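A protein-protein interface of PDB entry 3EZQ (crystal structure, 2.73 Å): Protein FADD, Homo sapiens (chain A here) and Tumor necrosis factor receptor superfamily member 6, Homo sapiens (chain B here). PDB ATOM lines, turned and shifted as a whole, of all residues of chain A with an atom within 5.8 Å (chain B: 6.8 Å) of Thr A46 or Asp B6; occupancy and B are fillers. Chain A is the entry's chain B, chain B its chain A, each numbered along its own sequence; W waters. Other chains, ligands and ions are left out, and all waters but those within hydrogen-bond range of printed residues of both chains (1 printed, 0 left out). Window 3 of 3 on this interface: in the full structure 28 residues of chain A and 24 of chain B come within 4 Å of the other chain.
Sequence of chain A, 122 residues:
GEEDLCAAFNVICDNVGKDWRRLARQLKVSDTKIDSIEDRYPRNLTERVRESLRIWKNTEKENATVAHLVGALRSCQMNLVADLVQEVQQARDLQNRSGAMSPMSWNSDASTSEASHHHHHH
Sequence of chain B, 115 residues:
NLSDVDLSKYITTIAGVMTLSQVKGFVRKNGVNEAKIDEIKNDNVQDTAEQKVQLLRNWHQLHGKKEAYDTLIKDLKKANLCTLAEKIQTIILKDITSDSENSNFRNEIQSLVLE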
ATOM      1  N   ASN A  10       8.817  -5.653 -29.559  1.00  0.00           N
ATOM      2  CA  ASN A  10       9.756  -6.773 -29.632  1.00  0.00           C
ATOM      3  C   ASN A  10      11.118  -6.370 -30.177  1.00  0.00           C
ATOM      4  O   ASN A  10      12.142  -6.882 -29.734  1.00  0.00           O
ATOM      5  CB  ASN A  10       9.199  -7.889 -30.490  1.00  0.00           C
ATOM      6  CG  ASN A  10       8.046  -8.602 -29.846  1.00  0.00           C
ATOM      7  OD1 ASN A  10       7.900  -8.524 -28.632  1.00  0.00           O
ATOM      8  ND2 ASN A  10       7.207  -9.289 -30.641  1.00  0.00           N
ATOM      9  N   CYS A  13      12.708  -3.929 -27.252  1.00  0.00           N
ATOM     10  CA  CYS A  13      13.049  -4.727 -26.062  1.00  0.00           C
ATOM     11  C   CYS A  13      14.385  -5.450 -26.123  1.00  0.00           C
ATOM     12  O   CYS A  13      15.149  -5.456 -25.162  1.00  0.00           O
ATOM     13  CB  CYS A  13      11.965  -5.773 -25.813  1.00  0.00           C
ATOM     14  SG  CYS A  13      10.645  -5.137 -24.798  1.00  0.00           S
ATOM     15  N   ASP A  14      14.651  -6.072 -27.259  1.00  0.00           N
ATOM     16  CA  ASP A  14      15.793  -6.947 -27.398  1.00  0.00           C
ATOM     17  C   ASP A  14      17.005  -6.192 -27.924  1.00  0.00           C
ATOM     18  O   ASP A  14      18.035  -6.802 -28.186  1.00  0.00           O
ATOM     19  CB  ASP A  14      15.441  -8.074 -28.389  1.00  0.00           C
ATOM     20  CG  ASP A  14      16.070  -9.404 -28.024  1.00  0.00           C
ATOM     21  OD1 ASP A  14      16.823  -9.971 -28.846  1.00  0.00           O
ATOM     22  OD2 ASP A  14      15.792  -9.895 -26.914  1.00  0.00           O
ATOM     23  N   ASN A  44      16.016  -9.137 -15.469  1.00  0.00           N
ATOM     24  CA  ASN A  44      16.215  -8.922 -16.899  1.00  0.00           C
ATOM     25  C   ASN A  44      16.039  -7.490 -17.428  1.00  0.00           C
ATOM     26  O   ASN A  44      14.974  -6.892 -17.286  1.00  0.00           O
ATOM     27  CB  ASN A  44      15.322  -9.898 -17.673  1.00  0.00           C
ATOM     28  CG  ASN A  44      15.802 -11.342 -17.645  1.00  0.00           C
ATOM     29  OD1 ASN A  44      16.758 -11.686 -18.329  1.00  0.00           O
ATOM     30  ND2 ASN A  44      15.129 -12.178 -16.860  1.00  0.00           N
ATOM     31  N   LEU A  45      17.111  -6.962 -18.015  1.00  0.00           N
ATOM     32  CA  LEU A  45      17.104  -5.637 -18.625  1.00  0.00           C
ATOM     33  C   LEU A  45      16.035  -5.526 -19.699  1.00  0.00           C
ATOM     34  O   LEU A  45      15.408  -4.477 -19.842  1.00  0.00           O
ATOM     35  CB  LEU A  45      18.485  -5.313 -19.207  1.00  0.00           C
ATOM     36  CG  LEU A  45      19.579  -5.140 -18.137  1.00  0.00           C
ATOM     37  CD1 LEU A  45      20.356  -6.434 -17.823  1.00  0.00           C
ATOM     38  CD2 LEU A  45      20.538  -4.019 -18.531  1.00  0.00           C
ATOM     39  N   THR A  46      15.824  -6.612 -20.439  1.00  0.00           N
ATOM     40  CA  THR A  46      14.825  -6.649 -21.518  1.00  0.00           C
ATOM     41  C   THR A  46      13.394  -6.524 -20.987  1.00  0.00           C
ATOM     42  O   THR A  46      12.528  -5.928 -21.641  1.00  0.00           O
ATOM     43  CB  THR A  46      14.925  -7.977 -22.336  1.00  0.00           C
ATOM     44  OG1 THR A  46      14.962  -9.092 -21.434  1.00  0.00           O
ATOM     45  CG2 THR A  46      16.174  -8.005 -23.210  1.00  0.00           C
ATOM     46  N   GLU A  47      13.153  -7.089 -19.809  1.00  0.00           N
ATOM     47  CA  GLU A  47      11.838  -7.045 -19.188  1.00  0.00           C
ATOM     48  C   GLU A  47      11.524  -5.637 -18.674  1.00  0.00           C
ATOM     49  O   GLU A  47      10.365  -5.208 -18.680  1.00  0.00           O
ATOM     50  CB  GLU A  47      11.804  -8.055 -18.041  1.00  0.00           C
ATOM     51  CG  GLU A  47      10.448  -8.304 -17.421  1.00  0.00           C
ATOM     52  CD  GLU A  47      10.518  -9.259 -16.223  1.00  0.00           C
ATOM     53  OE1 GLU A  47      11.582  -9.354 -15.562  1.00  0.00           O
ATOM     54  OE2 GLU A  47       9.493  -9.908 -15.933  1.00  0.00           O
ATOM     55  N   ARG A  48      12.561  -4.926 -18.234  1.00  0.00           N
ATOM     56  CA  ARG A  48      12.409  -3.552 -17.753  1.00  0.00           C
ATOM     57  C   ARG A  48      12.028  -2.618 -18.892  1.00  0.00           C
ATOM     58  O   ARG A  48      11.177  -1.743 -18.736  1.00  0.00           O
ATOM     59  CB  ARG A  48      13.702  -3.066 -17.094  1.00  0.00           C
ATOM     60  CG  ARG A  48      14.046  -3.799 -15.804  1.00  0.00           C
ATOM     61  CD  ARG A  48      14.988  -2.994 -14.929  1.00  0.00           C
ATOM     62  NE  ARG A  48      16.258  -2.683 -15.592  1.00  0.00           N
ATOM     63  CZ  ARG A  48      17.389  -3.380 -15.472  1.00  0.00           C
ATOM     64  NH1 ARG A  48      17.459  -4.484 -14.720  1.00  0.00           N
ATOM     65  NH2 ARG A  48      18.470  -2.962 -16.126  1.00  0.00           N
ATOM     66  N   VAL A  49      12.670  -2.820 -20.037  1.00  0.00           N
ATOM     67  CA  VAL A  49      12.381  -2.053 -21.239  1.00  0.00           C
ATOM     68  C   VAL A  49      10.917  -2.230 -21.668  1.00  0.00           C
ATOM     69  O   VAL A  49      10.238  -1.252 -21.989  1.00  0.00           O
ATOM     70  CB  VAL A  49      13.303  -2.499 -22.413  1.00  0.00           C
ATOM     71  CG1 VAL A  49      12.979  -1.719 -23.706  1.00  0.00           C
ATOM     72  CG2 VAL A  49      14.773  -2.346 -22.039  1.00  0.00           C
ATOM     73  N   ARG A  50      10.432  -3.472 -21.660  1.00  0.00           N
ATOM     74  CA  ARG A  50       9.057  -3.757 -22.086  1.00  0.00           C
ATOM     75  C   ARG A  50       8.015  -3.050 -21.217  1.00  0.00           C
ATOM     76  O   ARG A  50       7.091  -2.434 -21.748  1.00  0.00           O
ATOM     77  CB  ARG A  50       8.760  -5.262 -22.084  1.00  0.00           C
ATOM     78  CG  ARG A  50       7.457  -5.612 -22.819  1.00  0.00           C
ATOM     79  CD  ARG A  50       7.072  -7.101 -22.708  1.00  0.00           C
ATOM     80  NE  ARG A  50       8.001  -7.980 -23.414  1.00  0.00           N
ATOM     81  CZ  ARG A  50       8.125  -8.040 -24.739  1.00  0.00           C
ATOM     82  NH1 ARG A  50       7.388  -7.265 -25.538  1.00  0.00           N
ATOM     83  NH2 ARG A  50       9.006  -8.876 -25.274  1.00  0.00           N
ATOM     84  N   GLU A  51       8.148  -3.151 -19.896  1.00  0.00           N
ATOM     85  CA  GLU A  51       7.174  -2.535 -18.987  1.00  0.00           C
ATOM     86  C   GLU A  51       7.133  -1.009 -19.139  1.00  0.00           C
ATOM     87  O   GLU A  51       6.065  -0.404 -19.020  1.00  0.00           O
ATOM     88  CB  GLU A  51       7.456  -2.930 -17.532  1.00  0.00           C
ATOM     89  CG  GLU A  51       6.355  -2.551 -16.524  1.00  0.00           C
ATOM     90  CD  GLU A  51       5.065  -3.366 -16.676  1.00  0.00           C
ATOM     91  OE1 GLU A  51       4.452  -3.340 -17.764  1.00  0.00           O
ATOM     92  OE2 GLU A  51       4.651  -4.019 -15.696  1.00  0.00           O
ATOM     93  N   LEU B   2      14.849 -14.738 -19.113  1.00  0.00           N
ATOM     94  CA  LEU B   2      13.980 -14.500 -20.288  1.00  0.00           C
ATOM     95  C   LEU B   2      14.767 -14.060 -21.516  1.00  0.00           C
ATOM     96  O   LEU B   2      14.190 -13.650 -22.535  1.00  0.00           O
ATOM     97  CB  LEU B   2      12.898 -13.440 -20.003  1.00  0.00           C
ATOM     98  CG  LEU B   2      11.727 -13.778 -19.048  1.00  0.00           C
ATOM     99  CD1 LEU B   2      10.556 -12.749 -19.217  1.00  0.00           C
ATOM    100  CD2 LEU B   2      11.227 -15.192 -19.297  1.00  0.00           C
ATOM    101  N   SER B   3      16.089 -14.142 -21.433  1.00  0.00           N
ATOM    102  CA  SER B   3      16.917 -13.692 -22.528  1.00  0.00           C
ATOM    103  C   SER B   3      16.490 -14.368 -23.820  1.00  0.00           C
ATOM    104  O   SER B   3      16.316 -13.708 -24.839  1.00  0.00           O
ATOM    105  CB  SER B   3      18.374 -14.007 -22.226  1.00  0.00           C
ATOM    106  OG  SER B   3      19.205 -13.450 -23.221  1.00  0.00           O
ATOM    107  N   ASP B   4      16.312 -15.683 -23.777  1.00  0.00           N
ATOM    108  CA  ASP B   4      15.988 -16.437 -24.985  1.00  0.00           C
ATOM    109  C   ASP B   4      14.530 -16.288 -25.445  1.00  0.00           C
ATOM    110  O   ASP B   4      14.247 -16.444 -26.636  1.00  0.00           O
ATOM    111  CB  ASP B   4      16.331 -17.927 -24.825  1.00  0.00           C
ATOM    112  CG  ASP B   4      16.299 -18.672 -26.163  1.00  0.00           C
ATOM    113  OD1 ASP B   4      17.264 -18.546 -26.957  1.00  0.00           O
ATOM    114  OD2 ASP B   4      15.278 -19.366 -26.439  1.00  0.00           O
ATOM    115  N   VAL B   5      13.608 -16.015 -24.523  1.00  0.00           N
ATOM    116  CA  VAL B   5      12.224 -15.770 -24.918  1.00  0.00           C
ATOM    117  C   VAL B   5      12.155 -14.445 -25.666  1.00  0.00           C
ATOM    118  O   VAL B   5      11.539 -14.335 -26.747  1.00  0.00           O
ATOM    119  CB  VAL B   5      11.255 -15.664 -23.747  1.00  0.00           C
ATOM    120  CG1 VAL B   5       9.908 -15.066 -24.226  1.00  0.00           C
ATOM    121  CG2 VAL B   5      11.058 -17.045 -23.052  1.00  0.00           C
ATOM    122  N   ASP B   6      12.792 -13.423 -25.106  1.00  0.00           N
ATOM    123  CA  ASP B   6      12.785 -12.124 -25.754  1.00  0.00           C
ATOM    124  C   ASP B   6      13.549 -12.170 -27.058  1.00  0.00           C
ATOM    125  O   ASP B   6      13.158 -11.504 -28.017  1.00  0.00           O
ATOM    126  CB  ASP B   6      13.318 -11.035 -24.835  1.00  0.00           C
ATOM    127  CG  ASP B   6      12.392 -10.766 -23.671  1.00  0.00           C
ATOM    128  OD1 ASP B   6      11.153 -10.836 -23.849  1.00  0.00           O
ATOM    129  OD2 ASP B   6      12.906 -10.485 -22.566  1.00  0.00           O
ATOM    130  N   LEU B   7      14.619 -12.955 -27.126  1.00  0.00           N
ATOM    131  CA  LEU B   7      15.326 -13.105 -28.407  1.00  0.00           C
ATOM    132  C   LEU B   7      14.414 -13.813 -29.389  1.00  0.00           C
ATOM    133  O   LEU B   7      14.425 -13.503 -30.569  1.00  0.00           O
ATOM    134  CB  LEU B   7      16.625 -13.889 -28.266  1.00  0.00           C
ATOM    135  CG  LEU B   7      17.261 -14.354 -29.579  1.00  0.00           C
ATOM    136  CD1 LEU B   7      17.831 -13.184 -30.334  1.00  0.00           C
ATOM    137  CD2 LEU B   7      18.334 -15.404 -29.294  1.00  0.00           C
ATOM    138  N   SER B   8      13.630 -14.772 -28.908  1.00  0.00           N
ATOM    139  CA  SER B   8      12.706 -15.481 -29.786  1.00  0.00           C
ATOM    140  C   SER B   8      11.576 -14.584 -30.279  1.00  0.00           C
ATOM    141  O   SER B   8      11.220 -14.609 -31.464  1.00  0.00           O
ATOM    142  CB  SER B   8      12.066 -16.674 -29.116  1.00  0.00           C
ATOM    143  OG  SER B   8      10.942 -17.072 -29.903  1.00  0.00           O
ATOM    144  N   LYS B   9      10.988 -13.808 -29.381  1.00  0.00           N
ATOM    145  CA  LYS B   9       9.936 -12.875 -29.809  1.00  0.00           C
ATOM    146  C   LYS B   9      10.453 -11.927 -30.879  1.00  0.00           C
ATOM    147  O   LYS B   9       9.795 -11.685 -31.895  1.00  0.00           O
ATOM    148  CB  LYS B   9       9.381 -12.072 -28.639  1.00  0.00           C
ATOM    149  CG  LYS B   9       8.581 -12.921 -27.655  1.00  0.00           C
ATOM    150  CD  LYS B   9       8.066 -12.100 -26.491  1.00  0.00           C
ATOM    151  CE  LYS B   9       6.880 -12.818 -25.840  1.00  0.00           C
ATOM    152  NZ  LYS B   9       6.279 -12.051 -24.724  1.00  0.00           N
ATOM    153  N   TYR B  10      11.646 -11.393 -30.666  1.00  0.00           N
ATOM    154  CA  TYR B  10      12.270 -10.497 -31.649  1.00  0.00           C
ATOM    155  C   TYR B  10      12.498 -11.174 -32.988  1.00  0.00           C
ATOM    156  O   TYR B  10      12.028 -10.707 -33.994  1.00  0.00           O
ATOM    157  CB  TYR B  10      13.599  -9.985 -31.115  1.00  0.00           C
ATOM    158  CG  TYR B  10      14.475  -9.298 -32.123  1.00  0.00           C
ATOM    159  CD1 TYR B  10      13.970  -8.303 -32.944  1.00  0.00           C
ATOM    160  CD2 TYR B  10      15.826  -9.604 -32.216  1.00  0.00           C
ATOM    161  CE1 TYR B  10      14.773  -7.657 -33.844  1.00  0.00           C
ATOM    162  CE2 TYR B  10      16.642  -8.950 -33.119  1.00  0.00           C
ATOM    163  CZ  TYR B  10      16.108  -7.977 -33.930  1.00  0.00           C
ATOM    164  OH  TYR B  10      16.902  -7.331 -34.847  1.00  0.00           O
ATOM    165  N   ILE B  11      13.222 -12.284 -33.007  1.00  0.00           N
ATOM    166  CA  ILE B  11      13.504 -12.966 -34.278  1.00  0.00           C
ATOM    167  C   ILE B  11      12.243 -13.470 -34.957  1.00  0.00           C
ATOM    168  O   ILE B  11      12.199 -13.570 -36.162  1.00  0.00           O
ATOM    169  CB  ILE B  11      14.501 -14.118 -34.097  1.00  0.00           C
ATOM    170  CG1 ILE B  11      15.923 -13.555 -34.123  1.00  0.00           C
ATOM    171  CG2 ILE B  11      14.334 -15.163 -35.195  1.00  0.00           C
ATOM    172  CD1 ILE B  11      16.926 -14.434 -33.438  1.00  0.00           C
HETATM  173  O   HOH W   1      12.060  -9.357 -28.437  1.00  0.00           O
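OD1 of Asp B6 lies within salt-bridge range of NH2 of Arg A50 (3.2 Å). The side-chain carboxylate (OD2) of Asp B6 lies within hydrogen-bond range of the side-chain hydroxyl (OG1) of Thr A46 (2.7 Å). N of Leu B7 sits at hydrogen-bond distance from OD2 of Asp A14. The side-chain amide nitrogen (ND2) of Asn A44 sits close to the backbone NH (N) of Leu B2 (3.4 Å). The side-chain carboxylate (OD2) of Asp A14 lies close to the backbone carbonyl oxygen (O) of Asp B6 (3.3 Å).
NH1 of Arg A50 is in hydrogen-bond range of OD1 of Asn A10 (3.4 Å). The side-chain sulfur of Cys A13 is in hydrogen-bond range of the backbone carbonyl oxygen of Thr A46 (3.8 Å). The side-chain sulfur (SG) of Cys A13 lies close to the backbone NH (N) of Arg A50.
Asn A10 touches Lys B9. Tyr B10 touches Asn A10 (CB to O, 3.7 Å). CD2 of Tyr B10 touches OD1 of Asp A14, at 3.5 Å. NH2 of Arg A50 touches CD of Lys B9, at 3.6 Å.
Of the printed residues of chain B, Thr A46 touches Asp B6 (2.7 Å). Asp B6 touches three residues of chain A. Of the printed residues of chain A, Lys B9 touches Asn A10 and Arg A50. Of the printed residues of chain B, Asn A10 touches Lys B9 and Tyr B10. Of the printed residues of chain A, Tyr B10 touches Asn A10 and Asp A14. Of the printed residues of chain B, Asn A44 touches Leu B2. Asp B4 touches none of the printed residues of chain A. The nearest residue of chain A that does not touch Asp B6 is Glu A47 (4.4 Å). The nearest printed residue of chain B that does not touch Arg A50 is Val B5 (6.2 Å).
Of the 10 printed residues of chain B, 5 touch a printed residue of chain A. Printed residues of chain B that touch a printed residue of chain A: Leu B2, Asp B6, Leu B7, Lys B9 and Tyr B10. Among the printed residues, 9 pairs touch across the chains. Among the printed residues, Asp or Glu carboxylates within 4 Å of a Lys or Arg side-chain nitrogen of the other chain: Arg A50 with Asp B6 (3.2 Å).
Water W1 lies within hydrogen-bond range of the backbone carbonyl oxygen of Asp B6, the backbone carbonyl oxygen of Asn A10 and the backbone NH of Tyr B10.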
